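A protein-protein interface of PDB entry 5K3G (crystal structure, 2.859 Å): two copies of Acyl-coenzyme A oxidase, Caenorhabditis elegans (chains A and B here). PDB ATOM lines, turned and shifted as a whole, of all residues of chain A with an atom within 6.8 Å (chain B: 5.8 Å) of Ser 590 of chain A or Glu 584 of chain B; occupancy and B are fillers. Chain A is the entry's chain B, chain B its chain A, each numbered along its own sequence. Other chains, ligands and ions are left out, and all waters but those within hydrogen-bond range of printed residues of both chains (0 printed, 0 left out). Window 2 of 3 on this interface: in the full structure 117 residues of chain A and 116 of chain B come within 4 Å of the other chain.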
ATOM      1  N   LEU A 583     -12.600   3.752  -1.606  1.00  0.00           N
ATOM      2  CA  LEU A 583     -13.429   4.230  -2.707  1.00  0.00           C
ATOM      3  C   LEU A 583     -14.810   4.670  -2.248  1.00  0.00           C
ATOM      4  O   LEU A 583     -15.471   5.447  -2.945  1.00  0.00           O
ATOM      5  CB  LEU A 583     -13.584   3.131  -3.759  1.00  0.00           C
ATOM      6  CG  LEU A 583     -12.347   2.728  -4.555  1.00  0.00           C
ATOM      7  CD1 LEU A 583     -12.457   1.290  -5.026  1.00  0.00           C
ATOM      8  CD2 LEU A 583     -12.200   3.664  -5.733  1.00  0.00           C
ATOM      9  N   MET A 588     -10.528   7.905  -2.433  1.00  0.00           N
ATOM     10  CA  MET A 588      -9.668   7.460  -3.520  1.00  0.00           C
ATOM     11  C   MET A 588     -10.469   7.404  -4.811  1.00  0.00           C
ATOM     12  O   MET A 588     -11.660   7.079  -4.804  1.00  0.00           O
ATOM     13  CB  MET A 588      -9.055   6.078  -3.253  1.00  0.00           C
ATOM     14  CG  MET A 588      -7.820   6.077  -2.379  1.00  0.00           C
ATOM     15  SD  MET A 588      -6.939   4.504  -2.492  1.00  0.00           S
ATOM     16  CE  MET A 588      -5.999   4.741  -4.001  1.00  0.00           C
ATOM     17  N   SER A 589      -9.804   7.713  -5.919  1.00  0.00           N
ATOM     18  CA  SER A 589     -10.426   7.677  -7.233  1.00  0.00           C
ATOM     19  C   SER A 589     -10.029   6.412  -7.987  1.00  0.00           C
ATOM     20  O   SER A 589      -9.075   5.716  -7.631  1.00  0.00           O
ATOM     21  CB  SER A 589     -10.050   8.918  -8.045  1.00  0.00           C
ATOM     22  OG  SER A 589      -8.665   8.933  -8.355  1.00  0.00           O
ATOM     23  N   SER A 590     -10.797   6.116  -9.041  1.00  0.00           N
ATOM     24  CA  SER A 590     -10.468   4.998  -9.923  1.00  0.00           C
ATOM     25  C   SER A 590      -9.061   5.142 -10.491  1.00  0.00           C
ATOM     26  O   SER A 590      -8.304   4.166 -10.561  1.00  0.00           O
ATOM     27  CB  SER A 590     -11.506   4.915 -11.046  1.00  0.00           C
ATOM     28  OG  SER A 590     -11.355   3.756 -11.851  1.00  0.00           O
ATOM     29  N   THR A 591      -8.683   6.367 -10.875  1.00  0.00           N
ATOM     30  CA  THR A 591      -7.352   6.613 -11.424  1.00  0.00           C
ATOM     31  C   THR A 591      -6.264   6.258 -10.419  1.00  0.00           C
ATOM     32  O   THR A 591      -5.277   5.597 -10.762  1.00  0.00           O
ATOM     33  CB  THR A 591      -7.227   8.076 -11.863  1.00  0.00           C
ATOM     34  OG1 THR A 591      -7.889   8.247 -13.120  1.00  0.00           O
ATOM     35  CG2 THR A 591      -5.764   8.476 -12.016  1.00  0.00           C
ATOM     36  N   GLN A 592      -6.426   6.701  -9.169  1.00  0.00           N
ATOM     37  CA  GLN A 592      -5.450   6.365  -8.138  1.00  0.00           C
ATOM     38  C   GLN A 592      -5.372   4.861  -7.894  1.00  0.00           C
ATOM     39  O   GLN A 592      -4.301   4.346  -7.553  1.00  0.00           O
ATOM     40  CB  GLN A 592      -5.789   7.089  -6.839  1.00  0.00           C
ATOM     41  CG  GLN A 592      -5.653   8.593  -6.909  1.00  0.00           C
ATOM     42  CD  GLN A 592      -6.127   9.260  -5.633  1.00  0.00           C
ATOM     43  OE1 GLN A 592      -7.297   9.168  -5.271  1.00  0.00           O
ATOM     44  NE2 GLN A 592      -5.216   9.925  -4.940  1.00  0.00           N
ATOM     45  N   LEU A 593      -6.487   4.140  -8.057  1.00  0.00           N
ATOM     46  CA  LEU A 593      -6.460   2.691  -7.877  1.00  0.00           C
ATOM     47  C   LEU A 593      -5.691   2.010  -9.003  1.00  0.00           C
ATOM     48  O   LEU A 593      -5.008   1.002  -8.778  1.00  0.00           O
ATOM     49  CB  LEU A 593      -7.885   2.140  -7.790  1.00  0.00           C
ATOM     50  CG  LEU A 593      -8.048   0.801  -7.061  1.00  0.00           C
ATOM     51  CD1 LEU A 593      -7.369   0.873  -5.702  1.00  0.00           C
ATOM     52  CD2 LEU A 593      -9.510   0.420  -6.910  1.00  0.00           C
ATOM     53  N   ASP A 594      -5.815   2.528 -10.230  1.00  0.00           N
ATOM     54  CA  ASP A 594      -4.992   2.031 -11.326  1.00  0.00           C
ATOM     55  C   ASP A 594      -3.514   2.282 -11.065  1.00  0.00           C
ATOM     56  O   ASP A 594      -2.670   1.454 -11.423  1.00  0.00           O
ATOM     57  CB  ASP A 594      -5.414   2.686 -12.640  1.00  0.00           C
ATOM     58  CG  ASP A 594      -6.743   2.182 -13.145  1.00  0.00           C
ATOM     59  OD1 ASP A 594      -7.131   1.059 -12.764  1.00  0.00           O
ATOM     60  OD2 ASP A 594      -7.391   2.905 -13.929  1.00  0.00           O
ATOM     61  N   TYR A 595      -3.186   3.420 -10.447  1.00  0.00           N
ATOM     62  CA  TYR A 595      -1.808   3.663 -10.033  1.00  0.00           C
ATOM     63  C   TYR A 595      -1.334   2.583  -9.071  1.00  0.00           C
ATOM     64  O   TYR A 595      -0.230   2.044  -9.219  1.00  0.00           O
ATOM     65  CB  TYR A 595      -1.686   5.045  -9.386  1.00  0.00           C
ATOM     66  CG  TYR A 595      -0.315   5.337  -8.818  1.00  0.00           C
ATOM     67  CD1 TYR A 595       0.720   5.754  -9.639  1.00  0.00           C
ATOM     68  CD2 TYR A 595      -0.057   5.192  -7.459  1.00  0.00           C
ATOM     69  CE1 TYR A 595       1.976   6.025  -9.127  1.00  0.00           C
ATOM     70  CE2 TYR A 595       1.198   5.455  -6.938  1.00  0.00           C
ATOM     71  CZ  TYR A 595       2.211   5.872  -7.775  1.00  0.00           C
ATOM     72  OH  TYR A 595       3.460   6.135  -7.252  1.00  0.00           O
ATOM     73  N   ARG A 597      -2.440  -0.430  -8.801  1.00  0.00           N
ATOM     74  CA  ARG A 597      -2.280  -1.685  -9.528  1.00  0.00           C
ATOM     75  C   ARG A 597      -0.988  -1.699 -10.328  1.00  0.00           C
ATOM     76  O   ARG A 597      -0.244  -2.689 -10.298  1.00  0.00           O
ATOM     77  CB  ARG A 597      -3.474  -1.915 -10.447  1.00  0.00           C
ATOM     78  CG  ARG A 597      -4.765  -2.241  -9.726  1.00  0.00           C
ATOM     79  CD  ARG A 597      -5.864  -2.609 -10.705  1.00  0.00           C
ATOM     80  NE  ARG A 597      -7.117  -2.938 -10.033  1.00  0.00           N
ATOM     81  CZ  ARG A 597      -8.150  -2.107  -9.936  1.00  0.00           C
ATOM     82  NH1 ARG A 597      -8.080  -0.897 -10.473  1.00  0.00           N
ATOM     83  NH2 ARG A 597      -9.254  -2.486  -9.308  1.00  0.00           N
ATOM     84  N   ARG B 501     -16.880  -4.849 -17.152  1.00  0.00           N
ATOM     85  CA  ARG B 501     -15.904  -3.769 -17.058  1.00  0.00           C
ATOM     86  C   ARG B 501     -14.504  -4.313 -16.810  1.00  0.00           C
ATOM     87  O   ARG B 501     -13.530  -3.816 -17.384  1.00  0.00           O
ATOM     88  CB  ARG B 501     -16.297  -2.785 -15.960  1.00  0.00           C
ATOM     89  CG  ARG B 501     -15.805  -1.363 -16.203  1.00  0.00           C
ATOM     90  CD  ARG B 501     -15.918  -0.486 -14.960  1.00  0.00           C
ATOM     91  NE  ARG B 501     -14.712  -0.524 -14.127  1.00  0.00           N
ATOM     92  CZ  ARG B 501     -13.833   0.474 -14.041  1.00  0.00           C
ATOM     93  NH1 ARG B 501     -14.029   1.589 -14.727  1.00  0.00           N
ATOM     94  NH2 ARG B 501     -12.758   0.363 -13.269  1.00  0.00           N
ATOM     95  N   LYS B 505     -11.476  -4.060 -19.342  1.00  0.00           N
ATOM     96  CA  LYS B 505     -10.341  -3.369 -18.744  1.00  0.00           C
ATOM     97  C   LYS B 505      -9.066  -4.195 -18.884  1.00  0.00           C
ATOM     98  O   LYS B 505      -8.045  -3.697 -19.357  1.00  0.00           O
ATOM     99  CB  LYS B 505     -10.615  -3.068 -17.270  1.00  0.00           C
ATOM    100  CG  LYS B 505      -9.880  -1.847 -16.739  1.00  0.00           C
ATOM    101  CD  LYS B 505      -9.593  -1.978 -15.252  1.00  0.00           C
ATOM    102  CE  LYS B 505      -8.558  -0.962 -14.798  1.00  0.00           C
ATOM    103  NZ  LYS B 505      -9.167   0.370 -14.532  1.00  0.00           N
ATOM    104  N   ALA B 579     -17.280  -5.418  -4.322  1.00  0.00           N
ATOM    105  CA  ALA B 579     -17.859  -4.081  -4.401  1.00  0.00           C
ATOM    106  C   ALA B 579     -16.911  -3.088  -5.064  1.00  0.00           C
ATOM    107  O   ALA B 579     -17.361  -2.131  -5.706  1.00  0.00           O
ATOM    108  CB  ALA B 579     -18.246  -3.594  -3.005  1.00  0.00           C
ATOM    109  N   THR B 580     -15.598  -3.289  -4.908  1.00  0.00           N
ATOM    110  CA  THR B 580     -14.599  -2.395  -5.493  1.00  0.00           C
ATOM    111  C   THR B 580     -14.884  -2.098  -6.959  1.00  0.00           C
ATOM    112  O   THR B 580     -14.862  -0.942  -7.390  1.00  0.00           O
ATOM    113  CB  THR B 580     -13.203  -3.012  -5.350  1.00  0.00           C
ATOM    114  OG1 THR B 580     -12.828  -3.024  -3.969  1.00  0.00           O
ATOM    115  CG2 THR B 580     -12.175  -2.210  -6.145  1.00  0.00           C
ATOM    116  N   TYR B 581     -15.171  -3.144  -7.734  1.00  0.00           N
ATOM    117  CA  TYR B 581     -15.395  -2.979  -9.164  1.00  0.00           C
ATOM    118  C   TYR B 581     -16.677  -2.206  -9.456  1.00  0.00           C
ATOM    119  O   TYR B 581     -16.754  -1.498 -10.466  1.00  0.00           O
ATOM    120  CB  TYR B 581     -15.428  -4.348  -9.839  1.00  0.00           C
ATOM    121  CG  TYR B 581     -14.201  -5.198  -9.574  1.00  0.00           C
ATOM    122  CD1 TYR B 581     -13.033  -5.009 -10.297  1.00  0.00           C
ATOM    123  CD2 TYR B 581     -14.220  -6.203  -8.610  1.00  0.00           C
ATOM    124  CE1 TYR B 581     -11.909  -5.781 -10.063  1.00  0.00           C
ATOM    125  CE2 TYR B 581     -13.099  -6.983  -8.371  1.00  0.00           C
ATOM    126  CZ  TYR B 581     -11.948  -6.766  -9.099  1.00  0.00           C
ATOM    127  OH  TYR B 581     -10.829  -7.533  -8.867  1.00  0.00           O
ATOM    128  N   ALA B 582     -17.685  -2.319  -8.590  1.00  0.00           N
ATOM    129  CA  ALA B 582     -18.915  -1.569  -8.804  1.00  0.00           C
ATOM    130  C   ALA B 582     -18.728  -0.100  -8.449  1.00  0.00           C
ATOM    131  O   ALA B 582     -19.282   0.782  -9.117  1.00  0.00           O
ATOM    132  CB  ALA B 582     -20.051  -2.178  -7.990  1.00  0.00           C
ATOM    133  N   LEU B 583     -17.939   0.181  -7.409  1.00  0.00           N
ATOM    134  CA  LEU B 583     -17.734   1.553  -6.956  1.00  0.00           C
ATOM    135  C   LEU B 583     -16.746   2.323  -7.822  1.00  0.00           C
ATOM    136  O   LEU B 583     -16.767   3.560  -7.826  1.00  0.00           O
ATOM    137  CB  LEU B 583     -17.225   1.560  -5.515  1.00  0.00           C
ATOM    138  CG  LEU B 583     -18.172   1.079  -4.421  1.00  0.00           C
ATOM    139  CD1 LEU B 583     -17.391   0.514  -3.254  1.00  0.00           C
ATOM    140  CD2 LEU B 583     -19.028   2.241  -3.979  1.00  0.00           C
ATOM    141  N   GLU B 584     -15.883   1.619  -8.557  1.00  0.00           N
ATOM    142  CA  GLU B 584     -14.730   2.268  -9.168  1.00  0.00           C
ATOM    143  C   GLU B 584     -15.134   3.285 -10.229  1.00  0.00           C
ATOM    144  O   GLU B 584     -14.468   4.314 -10.386  1.00  0.00           O
ATOM    145  CB  GLU B 584     -13.801   1.205  -9.753  1.00  0.00           C
ATOM    146  CG  GLU B 584     -12.335   1.589  -9.740  1.00  0.00           C
ATOM    147  CD  GLU B 584     -11.443   0.493 -10.274  1.00  0.00           C
ATOM    148  OE1 GLU B 584     -11.544  -0.645  -9.774  1.00  0.00           O
ATOM    149  OE2 GLU B 584     -10.652   0.767 -11.200  1.00  0.00           O
ATOM    150  N   ASP B 585     -16.219   3.034 -10.961  1.00  0.00           N
ATOM    151  CA  ASP B 585     -16.641   3.937 -12.026  1.00  0.00           C
ATOM    152  C   ASP B 585     -17.966   4.625 -11.716  1.00  0.00           C
ATOM    153  O   ASP B 585     -18.646   5.091 -12.636  1.00  0.00           O
ATOM    154  CB  ASP B 585     -16.737   3.185 -13.354  1.00  0.00           C
ATOM    155  CG  ASP B 585     -17.813   2.122 -13.341  1.00  0.00           C
ATOM    156  OD1 ASP B 585     -18.182   1.663 -12.244  1.00  0.00           O
ATOM    157  OD2 ASP B 585     -18.299   1.754 -14.431  1.00  0.00           O
ATOM    158  N   GLY B 586     -18.354   4.683 -10.443  1.00  0.00           N
ATOM    159  CA  GLY B 586     -19.596   5.334 -10.074  1.00  0.00           C
ATOM    160  C   GLY B 586     -20.848   4.535 -10.358  1.00  0.00           C
ATOM    161  O   GLY B 586     -21.954   5.045 -10.148  1.00  0.00           O
ATOM    162  N   PHE B 587     -20.710   3.294 -10.831  1.00  0.00           N
ATOM    163  CA  PHE B 587     -21.883   2.485 -11.141  1.00  0.00           C
ATOM    164  C   PHE B 587     -22.692   2.168  -9.890  1.00  0.00           C
ATOM    165  O   PHE B 587     -23.915   2.015  -9.970  1.00  0.00           O
ATOM    166  CB  PHE B 587     -21.466   1.196 -11.844  1.00  0.00           C
ATOM    167  CG  PHE B 587     -22.611   0.428 -12.425  1.00  0.00           C
ATOM    168  CD1 PHE B 587     -23.133   0.771 -13.660  1.00  0.00           C
ATOM    169  CD2 PHE B 587     -23.173  -0.635 -11.737  1.00  0.00           C
ATOM    170  CE1 PHE B 587     -24.195   0.066 -14.199  1.00  0.00           C
ATOM    171  CE2 PHE B 587     -24.231  -1.348 -12.273  1.00  0.00           C
ATOM    172  CZ  PHE B 587     -24.747  -0.994 -13.502  1.00  0.00           C
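Of the 11 printed residues of chain B, 4 touch a printed residue of chain A.
Printed residues of chain B that touch a printed residue of chain A: Arg 501, Lys 505, Thr 580 and Glu 584.
Of the 10 printed residues of chain A, 5 touch a printed residue of chain B.
Among the printed residues, 8 pairs touch across the chains.
Among the printed residues, Asp or Glu carboxylates within 4 Å of a Lys or Arg side-chain nitrogen of the other chain: Asp 594 of chain A with Lys 505 of chain B (2.8 Å) and Arg 597 of chain A with Glu 584 of chain B (3.0 Å).
Of chain B, only Arg 501 and Glu 584 come within 4 Å of Ser 590 of chain A.
Glu 584 of chain B touches four residues of chain A.
Of the printed residues of chain B, Leu 593 of chain A touches Thr 580 (3.8 Å) and Glu 584 (3.7 Å).
Printed residues of chain A within 4 Å of Thr 580 of chain B: Leu 583 and Leu 593.
Of the printed residues of chain A, Lys 505 of chain B touches Asp 594 (2.8 Å).
Met 588 of chain A touches none of the printed residues of chain B.
The nearest printed residue of chain B that does not touch Asp 594 of chain A is Arg 501 of chain B (5.7 Å).
Among the printed residues, pairs that only touch across the chains: Leu 583 of chain A with Thr 580 of chain B (3.7 Å), Ser 590 of chain A with Arg 501 of chain B (3.9 Å), Leu 593 of chain A with Thr 580 of chain B (3.8 Å), Leu 593 of chain A with Glu 584 of chain B (3.7 Å) and Asp 594 of chain A with Glu 584 of chain B (3.9 Å).
NZ of Lys 505 of chain B lies within salt-bridge range of OD1 of Asp 594 of chain A (2.8 Å).
NH2 of Arg 597 of chain A is in salt-bridge range of OE1 of Glu 584 of chain B (3.0 Å).
The side-chain carboxylate (OE2) of Glu 584 of chain B sits at hydrogen-bond distance from the side-chain hydroxyl (OG) of Ser 590 of chain A, 3.1 Å away.
Position printed for both chains: 583.
Of the 8 pairs that touch across the chains among the printed residues, none has its exchanged pair printed and touching as well.
NZ of Lys 505 of chain B is in salt-bridge range of OE2 of Glu 584 of chain B, 3.7 Å away.
OD1 of Asp 594 of chain A lies within salt-bridge range of NH1 of Arg 597 of chain A.
The guanidinium group (NH2) of Arg 501 of chain B lies within salt-bridge range of the side-chain carboxylate (OE2) of Glu 584 of chain B, 3.0 Å away.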
